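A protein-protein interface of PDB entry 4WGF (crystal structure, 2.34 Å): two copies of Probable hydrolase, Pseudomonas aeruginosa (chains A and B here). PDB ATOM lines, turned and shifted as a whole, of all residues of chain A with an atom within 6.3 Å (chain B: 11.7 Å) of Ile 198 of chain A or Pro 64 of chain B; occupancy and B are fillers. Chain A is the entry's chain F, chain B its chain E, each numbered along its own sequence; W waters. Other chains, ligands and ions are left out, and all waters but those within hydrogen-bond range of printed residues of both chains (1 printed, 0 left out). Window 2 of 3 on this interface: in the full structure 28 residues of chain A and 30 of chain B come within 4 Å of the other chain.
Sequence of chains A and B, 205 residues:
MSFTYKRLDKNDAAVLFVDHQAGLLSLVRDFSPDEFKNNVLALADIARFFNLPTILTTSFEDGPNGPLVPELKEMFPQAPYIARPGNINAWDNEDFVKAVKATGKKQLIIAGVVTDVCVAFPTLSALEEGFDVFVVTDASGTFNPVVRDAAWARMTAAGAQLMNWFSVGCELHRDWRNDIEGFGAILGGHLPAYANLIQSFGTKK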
ATOM      1  N   GLY A 184      -9.160  33.673 -15.501  1.00  0.00           N
ATOM      2  CA  GLY A 184      -8.705  32.345 -15.130  1.00  0.00           C
ATOM      3  C   GLY A 184      -7.702  32.364 -13.993  1.00  0.00           C
ATOM      4  O   GLY A 184      -7.650  31.437 -13.185  1.00  0.00           O
ATOM      5  N   ALA A 185      -6.902  33.424 -13.932  1.00  0.00           N
ATOM      6  CA  ALA A 185      -5.904  33.578 -12.879  1.00  0.00           C
ATOM      7  C   ALA A 185      -6.566  33.797 -11.523  1.00  0.00           C
ATOM      8  O   ALA A 185      -6.056  33.349 -10.494  1.00  0.00           O
ATOM      9  CB  ALA A 185      -4.966  34.729 -13.204  1.00  0.00           C
ATOM     10  N   LEU A 187      -9.639  32.635 -10.677  1.00  0.00           N
ATOM     11  CA  LEU A 187     -10.218  31.343 -10.330  1.00  0.00           C
ATOM     12  C   LEU A 187      -9.142  30.375  -9.856  1.00  0.00           C
ATOM     13  O   LEU A 187      -9.307  29.699  -8.842  1.00  0.00           O
ATOM     14  CB  LEU A 187     -10.970  30.753 -11.527  1.00  0.00           C
ATOM     15  CG  LEU A 187     -12.466  31.058 -11.646  1.00  0.00           C
ATOM     16  CD1 LEU A 187     -12.748  32.548 -11.525  1.00  0.00           C
ATOM     17  CD2 LEU A 187     -13.012  30.516 -12.959  1.00  0.00           C
ATOM     18  N   GLY A 188      -8.038  30.316 -10.593  1.00  0.00           N
ATOM     19  CA  GLY A 188      -6.933  29.446 -10.240  1.00  0.00           C
ATOM     20  C   GLY A 188      -6.280  29.844  -8.931  1.00  0.00           C
ATOM     21  O   GLY A 188      -5.782  28.997  -8.192  1.00  0.00           O
ATOM     22  N   ALA A 193      -8.703  23.467  -6.511  1.00  0.00           N
ATOM     23  CA  ALA A 193      -9.133  22.389  -7.391  1.00  0.00           C
ATOM     24  C   ALA A 193      -9.115  22.844  -8.845  1.00  0.00           C
ATOM     25  O   ALA A 193      -8.829  22.057  -9.748  1.00  0.00           O
ATOM     26  CB  ALA A 193     -10.520  21.905  -7.001  1.00  0.00           C
ATOM     27  N   TYR A 194      -9.418  24.119  -9.066  1.00  0.00           N
ATOM     28  CA  TYR A 194      -9.435  24.674 -10.413  1.00  0.00           C
ATOM     29  C   TYR A 194      -8.014  24.939 -10.898  1.00  0.00           C
ATOM     30  O   TYR A 194      -7.723  24.819 -12.088  1.00  0.00           O
ATOM     31  CB  TYR A 194     -10.260  25.961 -10.466  1.00  0.00           C
ATOM     32  CG  TYR A 194     -10.712  26.316 -11.861  1.00  0.00           C
ATOM     33  CD1 TYR A 194     -11.853  25.741 -12.405  1.00  0.00           C
ATOM     34  CD2 TYR A 194      -9.989  27.207 -12.642  1.00  0.00           C
ATOM     35  CE1 TYR A 194     -12.270  26.053 -13.682  1.00  0.00           C
ATOM     36  CE2 TYR A 194     -10.398  27.524 -13.923  1.00  0.00           C
ATOM     37  CZ  TYR A 194     -11.540  26.944 -14.438  1.00  0.00           C
ATOM     38  OH  TYR A 194     -11.957  27.254 -15.712  1.00  0.00           O
ATOM     39  N   ALA A 195      -7.137  25.307  -9.969  1.00  0.00           N
ATOM     40  CA  ALA A 195      -5.724  25.476 -10.278  1.00  0.00           C
ATOM     41  C   ALA A 195      -5.144  24.154 -10.762  1.00  0.00           C
ATOM     42  O   ALA A 195      -4.298  24.121 -11.656  1.00  0.00           O
ATOM     43  CB  ALA A 195      -4.963  25.981  -9.061  1.00  0.00           C
ATOM     44  N   ASN A 196      -5.614  23.065 -10.161  1.00  0.00           N
ATOM     45  CA  ASN A 196      -5.189  21.726 -10.544  1.00  0.00           C
ATOM     46  C   ASN A 196      -5.643  21.365 -11.954  1.00  0.00           C
ATOM     47  O   ASN A 196      -4.904  20.734 -12.708  1.00  0.00           O
ATOM     48  CB  ASN A 196      -5.717  20.697  -9.544  1.00  0.00           C
ATOM     49  CG  ASN A 196      -5.089  20.843  -8.173  1.00  0.00           C
ATOM     50  OD1 ASN A 196      -3.958  21.311  -8.043  1.00  0.00           O
ATOM     51  ND2 ASN A 196      -5.824  20.446  -7.138  1.00  0.00           N
ATOM     52  N   LEU A 197      -6.865  21.762 -12.299  1.00  0.00           N
ATOM     53  CA  LEU A 197      -7.395  21.538 -13.640  1.00  0.00           C
ATOM     54  C   LEU A 197      -6.561  22.277 -14.678  1.00  0.00           C
ATOM     55  O   LEU A 197      -6.259  21.741 -15.745  1.00  0.00           O
ATOM     56  CB  LEU A 197      -8.854  21.987 -13.731  1.00  0.00           C
ATOM     57  CG  LEU A 197      -9.886  21.247 -12.880  1.00  0.00           C
ATOM     58  CD1 LEU A 197     -11.239  21.927 -12.999  1.00  0.00           C
ATOM     59  CD2 LEU A 197      -9.978  19.790 -13.293  1.00  0.00           C
ATOM     60  N   ILE A 198      -6.192  23.512 -14.353  1.00  0.00           N
ATOM     61  CA  ILE A 198      -5.391  24.336 -15.246  1.00  0.00           C
ATOM     62  C   ILE A 198      -4.015  23.715 -15.469  1.00  0.00           C
ATOM     63  O   ILE A 198      -3.528  23.659 -16.598  1.00  0.00           O
ATOM     64  CB  ILE A 198      -5.231  25.771 -14.699  1.00  0.00           C
ATOM     65  CG1 ILE A 198      -6.583  26.486 -14.680  1.00  0.00           C
ATOM     66  CG2 ILE A 198      -4.231  26.558 -15.530  1.00  0.00           C
ATOM     67  CD1 ILE A 198      -6.533  27.879 -14.088  1.00  0.00           C
ATOM     68  N   GLN A 199      -3.397  23.238 -14.392  1.00  0.00           N
ATOM     69  CA  GLN A 199      -2.063  22.656 -14.486  1.00  0.00           C
ATOM     70  C   GLN A 199      -2.062  21.355 -15.286  1.00  0.00           C
ATOM     71  O   GLN A 199      -1.170  21.128 -16.102  1.00  0.00           O
ATOM     72  CB  GLN A 199      -1.473  22.408 -13.096  1.00  0.00           C
ATOM     73  CG  GLN A 199      -0.009  21.992 -13.142  1.00  0.00           C
ATOM     74  CD  GLN A 199       0.534  21.568 -11.794  1.00  0.00           C
ATOM     75  OE1 GLN A 199      -0.207  21.452 -10.819  1.00  0.00           O
ATOM     76  NE2 GLN A 199       1.842  21.338 -11.731  1.00  0.00           N
ATOM     77  N   SER A 200      -3.053  20.502 -15.048  1.00  0.00           N
ATOM     78  CA  SER A 200      -3.169  19.249 -15.790  1.00  0.00           C
ATOM     79  C   SER A 200      -3.409  19.517 -17.272  1.00  0.00           C
ATOM     80  O   SER A 200      -2.869  18.823 -18.134  1.00  0.00           O
ATOM     81  CB  SER A 200      -4.295  18.382 -15.225  1.00  0.00           C
ATOM     82  OG  SER A 200      -3.970  17.896 -13.934  1.00  0.00           O
ATOM     83  N   PHE A 201      -4.227  20.525 -17.558  1.00  0.00           N
ATOM     84  CA  PHE A 201      -4.537  20.901 -18.931  1.00  0.00           C
ATOM     85  C   PHE A 201      -3.304  21.458 -19.636  1.00  0.00           C
ATOM     86  O   PHE A 201      -3.174  21.351 -20.856  1.00  0.00           O
ATOM     87  CB  PHE A 201      -5.672  21.927 -18.960  1.00  0.00           C
ATOM     88  CG  PHE A 201      -6.091  22.335 -20.343  1.00  0.00           C
ATOM     89  CD1 PHE A 201      -6.951  21.541 -21.085  1.00  0.00           C
ATOM     90  CD2 PHE A 201      -5.632  23.518 -20.899  1.00  0.00           C
ATOM     91  CE1 PHE A 201      -7.340  21.917 -22.357  1.00  0.00           C
ATOM     92  CE2 PHE A 201      -6.016  23.899 -22.171  1.00  0.00           C
ATOM     93  CZ  PHE A 201      -6.873  23.098 -22.900  1.00  0.00           C
ATOM     94  N   GLY A 202      -2.402  22.052 -18.863  1.00  0.00           N
ATOM     95  CA  GLY A 202      -1.211  22.672 -19.413  1.00  0.00           C
ATOM     96  C   GLY A 202      -0.113  21.697 -19.802  1.00  0.00           C
ATOM     97  O   GLY A 202       0.786  22.046 -20.568  1.00  0.00           O
ATOM     98  N   THR A 203      -0.181  20.477 -19.279  1.00  0.00           N
ATOM     99  CA  THR A 203       0.843  19.470 -19.552  1.00  0.00           C
ATOM    100  C   THR A 203       0.587  18.718 -20.856  1.00  0.00           C
ATOM    101  O   THR A 203      -0.545  18.645 -21.332  1.00  0.00           O
ATOM    102  CB  THR A 203       0.945  18.452 -18.401  1.00  0.00           C
ATOM    103  OG1 THR A 203      -0.295  17.746 -18.276  1.00  0.00           O
ATOM    104  CG2 THR A 203       1.245  19.163 -17.098  1.00  0.00           C
ATOM    105  N   ASP B  19     -23.546  22.018 -18.035  1.00  0.00           N
ATOM    106  CA  ASP B  19     -22.137  21.988 -17.646  1.00  0.00           C
ATOM    107  C   ASP B  19     -21.765  20.876 -16.664  1.00  0.00           C
ATOM    108  O   ASP B  19     -20.991  21.101 -15.734  1.00  0.00           O
ATOM    109  CB  ASP B  19     -21.736  23.341 -17.052  1.00  0.00           C
ATOM    110  CG  ASP B  19     -22.119  24.504 -17.945  1.00  0.00           C
ATOM    111  OD1 ASP B  19     -22.541  24.255 -19.094  1.00  0.00           O
ATOM    112  OD2 ASP B  19     -22.004  25.664 -17.499  1.00  0.00           O
ATOM    113  N   HIS B  20     -22.312  19.681 -16.865  1.00  0.00           N
ATOM    114  CA  HIS B  20     -21.835  18.510 -16.136  1.00  0.00           C
ATOM    115  C   HIS B  20     -20.550  18.012 -16.785  1.00  0.00           C
ATOM    116  O   HIS B  20     -20.534  16.961 -17.425  1.00  0.00           O
ATOM    117  CB  HIS B  20     -22.885  17.398 -16.116  1.00  0.00           C
ATOM    118  CG  HIS B  20     -24.067  17.695 -15.250  1.00  0.00           C
ATOM    119  ND1 HIS B  20     -25.263  18.157 -15.754  1.00  0.00           N
ATOM    120  CD2 HIS B  20     -24.237  17.596 -13.910  1.00  0.00           C
ATOM    121  CE1 HIS B  20     -26.120  18.330 -14.764  1.00  0.00           C
ATOM    122  NE2 HIS B  20     -25.522  17.997 -13.634  1.00  0.00           N
ATOM    123  N   GLN B  21     -19.473  18.772 -16.614  1.00  0.00           N
ATOM    124  CA  GLN B  21     -18.222  18.490 -17.305  1.00  0.00           C
ATOM    125  C   GLN B  21     -17.184  17.886 -16.365  1.00  0.00           C
ATOM    126  O   GLN B  21     -17.205  18.145 -15.165  1.00  0.00           O
ATOM    127  CB  GLN B  21     -17.688  19.769 -17.951  1.00  0.00           C
ATOM    128  CG  GLN B  21     -18.660  20.381 -18.954  1.00  0.00           C
ATOM    129  CD  GLN B  21     -18.363  21.836 -19.261  1.00  0.00           C
ATOM    130  OE1 GLN B  21     -19.231  22.698 -19.135  1.00  0.00           O
ATOM    131  NE2 GLN B  21     -17.132  22.115 -19.676  1.00  0.00           N
ATOM    132  N   ALA B  22     -16.278  17.090 -16.927  1.00  0.00           N
ATOM    133  CA  ALA B  22     -15.301  16.326 -16.150  1.00  0.00           C
ATOM    134  C   ALA B  22     -14.477  17.188 -15.196  1.00  0.00           C
ATOM    135  O   ALA B  22     -14.228  16.798 -14.055  1.00  0.00           O
ATOM    136  CB  ALA B  22     -14.376  15.563 -17.090  1.00  0.00           C
ATOM    137  N   GLY B  23     -14.057  18.357 -15.663  1.00  0.00           N
ATOM    138  CA  GLY B  23     -13.268  19.257 -14.843  1.00  0.00           C
ATOM    139  C   GLY B  23     -14.081  19.928 -13.754  1.00  0.00           C
ATOM    140  O   GLY B  23     -13.719  19.884 -12.577  1.00  0.00           O
ATOM    141  N   LEU B  24     -15.189  20.545 -14.151  1.00  0.00           N
ATOM    142  CA  LEU B  24     -16.031  21.309 -13.235  1.00  0.00           C
ATOM    143  C   LEU B  24     -16.588  20.457 -12.095  1.00  0.00           C
ATOM    144  O   LEU B  24     -16.883  20.971 -11.017  1.00  0.00           O
ATOM    145  CB  LEU B  24     -17.181  21.960 -14.004  1.00  0.00           C
ATOM    146  CG  LEU B  24     -16.774  23.001 -15.048  1.00  0.00           C
ATOM    147  CD1 LEU B  24     -17.996  23.541 -15.776  1.00  0.00           C
ATOM    148  CD2 LEU B  24     -15.982  24.129 -14.405  1.00  0.00           C
ATOM    149  N   LEU B  25     -16.733  19.159 -12.340  1.00  0.00           N
ATOM    150  CA  LEU B  25     -17.293  18.248 -11.344  1.00  0.00           C
ATOM    151  C   LEU B  25     -16.393  18.091 -10.122  1.00  0.00           C
ATOM    152  O   LEU B  25     -16.857  17.714  -9.047  1.00  0.00           O
ATOM    153  CB  LEU B  25     -17.559  16.878 -11.967  1.00  0.00           C
ATOM    154  CG  LEU B  25     -18.820  16.781 -12.825  1.00  0.00           C
ATOM    155  CD1 LEU B  25     -18.827  15.486 -13.609  1.00  0.00           C
ATOM    156  CD2 LEU B  25     -20.059  16.891 -11.959  1.00  0.00           C
ATOM    157  N   SER B  26     -15.105  18.373 -10.289  1.00  0.00           N
ATOM    158  CA  SER B  26     -14.161  18.280  -9.183  1.00  0.00           C
ATOM    159  C   SER B  26     -14.324  19.448  -8.215  1.00  0.00           C
ATOM    160  O   SER B  26     -13.755  19.446  -7.124  1.00  0.00           O
ATOM    161  CB  SER B  26     -12.723  18.223  -9.704  1.00  0.00           C
ATOM    162  OG  SER B  26     -12.349  19.449 -10.306  1.00  0.00           O
ATOM    163  N   LEU B  27     -15.106  20.445  -8.620  1.00  0.00           N
ATOM    164  CA  LEU B  27     -15.405  21.587  -7.763  1.00  0.00           C
ATOM    165  C   LEU B  27     -16.555  21.267  -6.814  1.00  0.00           C
ATOM    166  O   LEU B  27     -16.693  21.884  -5.759  1.00  0.00           O
ATOM    167  CB  LEU B  27     -15.749  22.819  -8.603  1.00  0.00           C
ATOM    168  CG  LEU B  27     -14.699  23.324  -9.592  1.00  0.00           C
ATOM    169  CD1 LEU B  27     -15.236  24.515 -10.375  1.00  0.00           C
ATOM    170  CD2 LEU B  27     -13.405  23.687  -8.875  1.00  0.00           C
ATOM    171  N   VAL B  28     -17.379  20.299  -7.202  1.00  0.00           N
ATOM    172  CA  VAL B  28     -18.545  19.911  -6.414  1.00  0.00           C
ATOM    173  C   VAL B  28     -18.146  19.173  -5.143  1.00  0.00           C
ATOM    174  O   VAL B  28     -17.612  18.065  -5.202  1.00  0.00           O
ATOM    175  CB  VAL B  28     -19.501  19.020  -7.229  1.00  0.00           C
ATOM    176  CG1 VAL B  28     -20.665  18.561  -6.363  1.00  0.00           C
ATOM    177  CG2 VAL B  28     -19.995  19.758  -8.463  1.00  0.00           C
ATOM    178  N   THR B  58     -22.434  23.007 -22.567  1.00  0.00           N
ATOM    179  CA  THR B  58     -21.160  23.034 -21.859  1.00  0.00           C
ATOM    180  C   THR B  58     -20.549  24.426 -21.904  1.00  0.00           C
ATOM    181  O   THR B  58     -20.910  25.245 -22.750  1.00  0.00           O
ATOM    182  CB  THR B  58     -20.156  22.029 -22.457  1.00  0.00           C
ATOM    183  OG1 THR B  58     -19.934  22.337 -23.838  1.00  0.00           O
ATOM    184  CG2 THR B  58     -20.680  20.607 -22.339  1.00  0.00           C
ATOM    185  N   SER B  59     -19.622  24.688 -20.990  1.00  0.00           N
ATOM    186  CA  SER B  59     -18.947  25.978 -20.933  1.00  0.00           C
ATOM    187  C   SER B  59     -17.439  25.821 -21.094  1.00  0.00           C
ATOM    188  O   SER B  59     -16.779  25.251 -20.224  1.00  0.00           O
ATOM    189  CB  SER B  59     -19.257  26.687 -19.614  1.00  0.00           C
ATOM    190  OG  SER B  59     -18.457  27.846 -19.457  1.00  0.00           O
ATOM    191  N   PHE B  60     -16.909  26.333 -22.202  1.00  0.00           N
ATOM    192  CA  PHE B  60     -15.468  26.342 -22.447  1.00  0.00           C
ATOM    193  C   PHE B  60     -14.894  24.932 -22.324  1.00  0.00           C
ATOM    194  O   PHE B  60     -13.911  24.712 -21.618  1.00  0.00           O
ATOM    195  CB  PHE B  60     -14.772  27.296 -21.470  1.00  0.00           C
ATOM    196  CG  PHE B  60     -13.446  27.818 -21.951  1.00  0.00           C
ATOM    197  CD1 PHE B  60     -12.836  27.293 -23.080  1.00  0.00           C
ATOM    198  CD2 PHE B  60     -12.806  28.840 -21.266  1.00  0.00           C
ATOM    199  CE1 PHE B  60     -11.615  27.777 -23.515  1.00  0.00           C
ATOM    200  CE2 PHE B  60     -11.586  29.327 -21.697  1.00  0.00           C
ATOM    201  CZ  PHE B  60     -10.990  28.796 -22.823  1.00  0.00           C
ATOM    202  N   GLU B  61     -15.515  23.984 -23.020  1.00  0.00           N
ATOM    203  CA  GLU B  61     -15.185  22.571 -22.867  1.00  0.00           C
ATOM    204  C   GLU B  61     -13.798  22.234 -23.406  1.00  0.00           C
ATOM    205  O   GLU B  61     -13.242  21.183 -23.089  1.00  0.00           O
ATOM    206  CB  GLU B  61     -16.236  21.702 -23.561  1.00  0.00           C
ATOM    207  CG  GLU B  61     -16.241  21.816 -25.076  1.00  0.00           C
ATOM    208  CD  GLU B  61     -17.300  20.944 -25.724  1.00  0.00           C
ATOM    209  OE1 GLU B  61     -18.295  20.609 -25.046  1.00  0.00           O
ATOM    210  OE2 GLU B  61     -17.137  20.590 -26.911  1.00  0.00           O
ATOM    211  N   ASP B  62     -13.242  23.128 -24.218  1.00  0.00           N
ATOM    212  CA  ASP B  62     -11.920  22.915 -24.796  1.00  0.00           C
ATOM    213  C   ASP B  62     -10.825  23.483 -23.898  1.00  0.00           C
ATOM    214  O   ASP B  62      -9.706  23.729 -24.347  1.00  0.00           O
ATOM    215  CB  ASP B  62     -11.838  23.546 -26.186  1.00  0.00           C
ATOM    216  CG  ASP B  62     -12.720  22.841 -27.197  1.00  0.00           C
ATOM    217  OD1 ASP B  62     -12.952  21.624 -27.038  1.00  0.00           O
ATOM    218  OD2 ASP B  62     -13.183  23.504 -28.149  1.00  0.00           O
ATOM    219  N   GLY B  63     -11.155  23.684 -22.627  1.00  0.00           N
ATOM    220  CA  GLY B  63     -10.195  24.155 -21.648  1.00  0.00           C
ATOM    221  C   GLY B  63     -10.194  23.287 -20.404  1.00  0.00           C
ATOM    222  O   GLY B  63     -10.615  22.132 -20.454  1.00  0.00           O
ATOM    223  N   PRO B  64      -9.713  23.841 -19.279  1.00  0.00           N
ATOM    224  CA  PRO B  64      -9.667  23.148 -17.986  1.00  0.00           C
ATOM    225  C   PRO B  64     -11.031  22.623 -17.531  1.00  0.00           C
ATOM    226  O   PRO B  64     -11.084  21.635 -16.798  1.00  0.00           O
ATOM    227  CB  PRO B  64      -9.164  24.233 -17.031  1.00  0.00           C
ATOM    228  CG  PRO B  64      -8.372  25.147 -17.895  1.00  0.00           C
ATOM    229  CD  PRO B  64      -9.098  25.178 -19.206  1.00  0.00           C
ATOM    230  N   ASN B  65     -12.109  23.277 -17.956  1.00  0.00           N
ATOM    231  CA  ASN B  65     -13.457  22.843 -17.601  1.00  0.00           C
ATOM    232  C   ASN B  65     -13.739  21.418 -18.065  1.00  0.00           C
ATOM    233  O   ASN B  65     -14.528  20.701 -17.451  1.00  0.00           O
ATOM    234  CB  ASN B  65     -14.503  23.799 -18.181  1.00  0.00           C
ATOM    235  CG  ASN B  65     -14.538  25.131 -17.457  1.00  0.00           C
ATOM    236  OD1 ASN B  65     -13.710  25.401 -16.589  1.00  0.00           O
ATOM    237  ND2 ASN B  65     -15.504  25.973 -17.811  1.00  0.00           N
ATOM    238  N   GLY B  66     -13.095  21.015 -19.154  1.00  0.00           N
ATOM    239  CA  GLY B  66     -13.172  19.640 -19.611  1.00  0.00           C
ATOM    240  C   GLY B  66     -14.439  19.313 -20.376  1.00  0.00           C
ATOM    241  O   GLY B  66     -15.348  20.136 -20.470  1.00  0.00           O
ATOM    242  N   PRO B  67     -14.501  18.095 -20.931  1.00  0.00           N
ATOM    243  CA  PRO B  67     -15.627  17.635 -21.746  1.00  0.00           C
ATOM    244  C   PRO B  67     -16.844  17.244 -20.916  1.00  0.00           C
ATOM    245  O   PRO B  67     -16.720  16.972 -19.721  1.00  0.00           O
ATOM    246  CB  PRO B  67     -15.053  16.411 -22.458  1.00  0.00           C
ATOM    247  CG  PRO B  67     -14.071  15.864 -21.481  1.00  0.00           C
ATOM    248  CD  PRO B  67     -13.460  17.062 -20.799  1.00  0.00           C
ATOM    249  N   LEU B  68     -18.007  17.222 -21.555  1.00  0.00           N
ATOM    250  CA  LEU B  68     -19.224  16.715 -20.936  1.00  0.00           C
ATOM    251  C   LEU B  68     -19.036  15.245 -20.579  1.00  0.00           C
ATOM    252  O   LEU B  68     -18.337  14.521 -21.287  1.00  0.00           O
ATOM    253  CB  LEU B  68     -20.420  16.892 -21.874  1.00  0.00           C
ATOM    254  CG  LEU B  68     -21.814  16.610 -21.310  1.00  0.00           C
ATOM    255  CD1 LEU B  68     -22.202  17.667 -20.287  1.00  0.00           C
ATOM    256  CD2 LEU B  68     -22.840  16.536 -22.430  1.00  0.00           C
ATOM    257  N   VAL B  69     -19.633  14.814 -19.472  1.00  0.00           N
ATOM    258  CA  VAL B  69     -19.552  13.415 -19.068  1.00  0.00           C
ATOM    259  C   VAL B  69     -20.096  12.519 -20.175  1.00  0.00           C
ATOM    260  O   VAL B  69     -21.117  12.834 -20.787  1.00  0.00           O
ATOM    261  CB  VAL B  69     -20.321  13.155 -17.757  1.00  0.00           C
ATOM    262  CG1 VAL B  69     -19.543  13.697 -16.577  1.00  0.00           C
ATOM    263  CG2 VAL B  69     -21.709  13.770 -17.816  1.00  0.00           C
ATOM    264  N   ARG B  84     -20.848  26.296 -25.328  1.00  0.00           N
ATOM    265  CA  ARG B  84     -20.696  27.732 -25.144  1.00  0.00           C
ATOM    266  C   ARG B  84     -19.232  28.077 -24.917  1.00  0.00           C
ATOM    267  O   ARG B  84     -18.674  27.753 -23.870  1.00  0.00           O
ATOM    268  CB  ARG B  84     -21.542  28.215 -23.966  1.00  0.00           C
ATOM    269  CG  ARG B  84     -22.932  27.607 -23.914  1.00  0.00           C
ATOM    270  CD  ARG B  84     -23.809  28.318 -22.898  1.00  0.00           C
ATOM    271  NE  ARG B  84     -23.130  28.504 -21.618  1.00  0.00           N
ATOM    272  CZ  ARG B  84     -23.050  27.576 -20.670  1.00  0.00           C
ATOM    273  NH1 ARG B  84     -23.604  26.386 -20.856  1.00  0.00           N
ATOM    274  NH2 ARG B  84     -22.415  27.837 -19.536  1.00  0.00           N
ATOM    275  N   PRO B  85     -18.602  28.735 -25.901  1.00  0.00           N
ATOM    276  CA  PRO B  85     -17.182  29.077 -25.776  1.00  0.00           C
ATOM    277  C   PRO B  85     -16.918  30.176 -24.748  1.00  0.00           C
ATOM    278  O   PRO B  85     -15.836  30.207 -24.161  1.00  0.00           O
ATOM    279  CB  PRO B  85     -16.814  29.551 -27.185  1.00  0.00           C
ATOM    280  CG  PRO B  85     -18.092  30.056 -27.752  1.00  0.00           C
ATOM    281  CD  PRO B  85     -19.163  29.164 -27.193  1.00  0.00           C
ATOM    282  N   VAL B 113     -23.706  22.315 -12.998  1.00  0.00           N
ATOM    283  CA  VAL B 113     -22.535  22.635 -12.187  1.00  0.00           C
ATOM    284  C   VAL B 113     -21.890  23.935 -12.670  1.00  0.00           C
ATOM    285  O   VAL B 113     -21.559  24.053 -13.848  1.00  0.00           O
ATOM    286  CB  VAL B 113     -21.488  21.498 -12.248  1.00  0.00           C
ATOM    287  CG1 VAL B 113     -20.215  21.888 -11.514  1.00  0.00           C
ATOM    288  CG2 VAL B 113     -22.062  20.198 -11.697  1.00  0.00           C
HETATM  289  O   HOH W   1      -9.272  19.601  -9.667  1.00  0.00           O
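The side-chain amide oxygen (OD1) of Asn 65 of chain B is in hydrogen-bond range of the side-chain hydroxyl (OH) of Tyr 194 of chain A (2.7 Å).
Water W1 bridges the backbone carbonyl oxygen (O) of Ala 193 of chain A (2.5 Å) and the side-chain hydroxyl (OG) of Ser 26 of chain B (3.1 Å).
Of the 25 printed residues of chain B, 7 touch a printed residue of chain A. Hydrophobic or aromatic side chains of chain B within 4 Å of the printed part of chain A: Leu 27 and Pro 64. Printed residues of chain A that touch a printed residue of chain B: Ala 193, Tyr 194, Leu 197, Ile 198 and Phe 201.
No position is printed for both chains. Of the 8 pairs that touch across the chains among the printed residues, none has its exchanged pair printed and touching as well.
O of Gly 23 of chain B is in hydrogen-bond range of OG of Ser 26 of chain B (2.7 Å). The backbone NH (N) of Gly 23 of chain B sits at hydrogen-bond distance from the backbone carbonyl oxygen (O) of Asn 65 of chain B (3.0 Å). The backbone carbonyl oxygen (O) of Ser 59 of chain B is in hydrogen-bond range of the side-chain amide nitrogen (ND2) of Asn 65 of chain B (2.8 Å). The backbone carbonyl oxygen (O) of Asn 65 of chain B sits at hydrogen-bond distance from the backbone NH (N) of Leu 24 of chain B (3.4 Å).
Ile 198 of chain A touches just one residue of chain B: Pro 64. Pro 64 of chain B touches two residues of chain A. No residue of chain B comes within 4 Å of Gly 188 of chain A. No residue of chain B comes within 4 Å of Ala 195 of chain A. No residue of chain B comes within 4 Å of Gln 199 of chain A. Phe 201 of chain A touches two residues of chain B. No residue of chain B comes within 4 Å of Gly 202 of chain A. Printed residues of chain A within 4 Å of Asp 62 of chain B: Phe 201. Of the printed residues of chain B, Tyr 194 of chain A touches Asn 65 (2.7 Å). Of the printed residues of chain A, Gly 23 of chain B touches Leu 197. Ser 59 of chain B touches none of the printed residues of chain A. Phe 60 of chain B touches none of the printed residues of chain A. The nearest residue of chain B that does not touch Ile 198 of chain A is Asn 65 of chain B (6.9 Å). The nearest residue of chain A that does not touch Pro 64 of chain B is Phe 201 of chain A (4.02 Å). The nearest printed residue of chain B that does not touch Ala 193 of chain A is Ser 26 of chain B (4.1 Å).
Among the printed residues, pairs that only touch across the chains: Ala 193 of chain A with Leu 27 of chain B (3.9 Å), Leu 197 of chain A with Gly 23 of chain B (3.2 Å), Leu 197 of chain A with Ser 26 of chain B (3.8 Å), Leu 197 of chain A with Pro 64 of chain B (3.8 Å), Ile 198 of chain A with Pro 64 of chain B (3.9 Å), Phe 201 of chain A with Asp 62 of chain B (3.2 Å) and Phe 201 of chain A with Gly 63 of chain B (3.7 Å).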
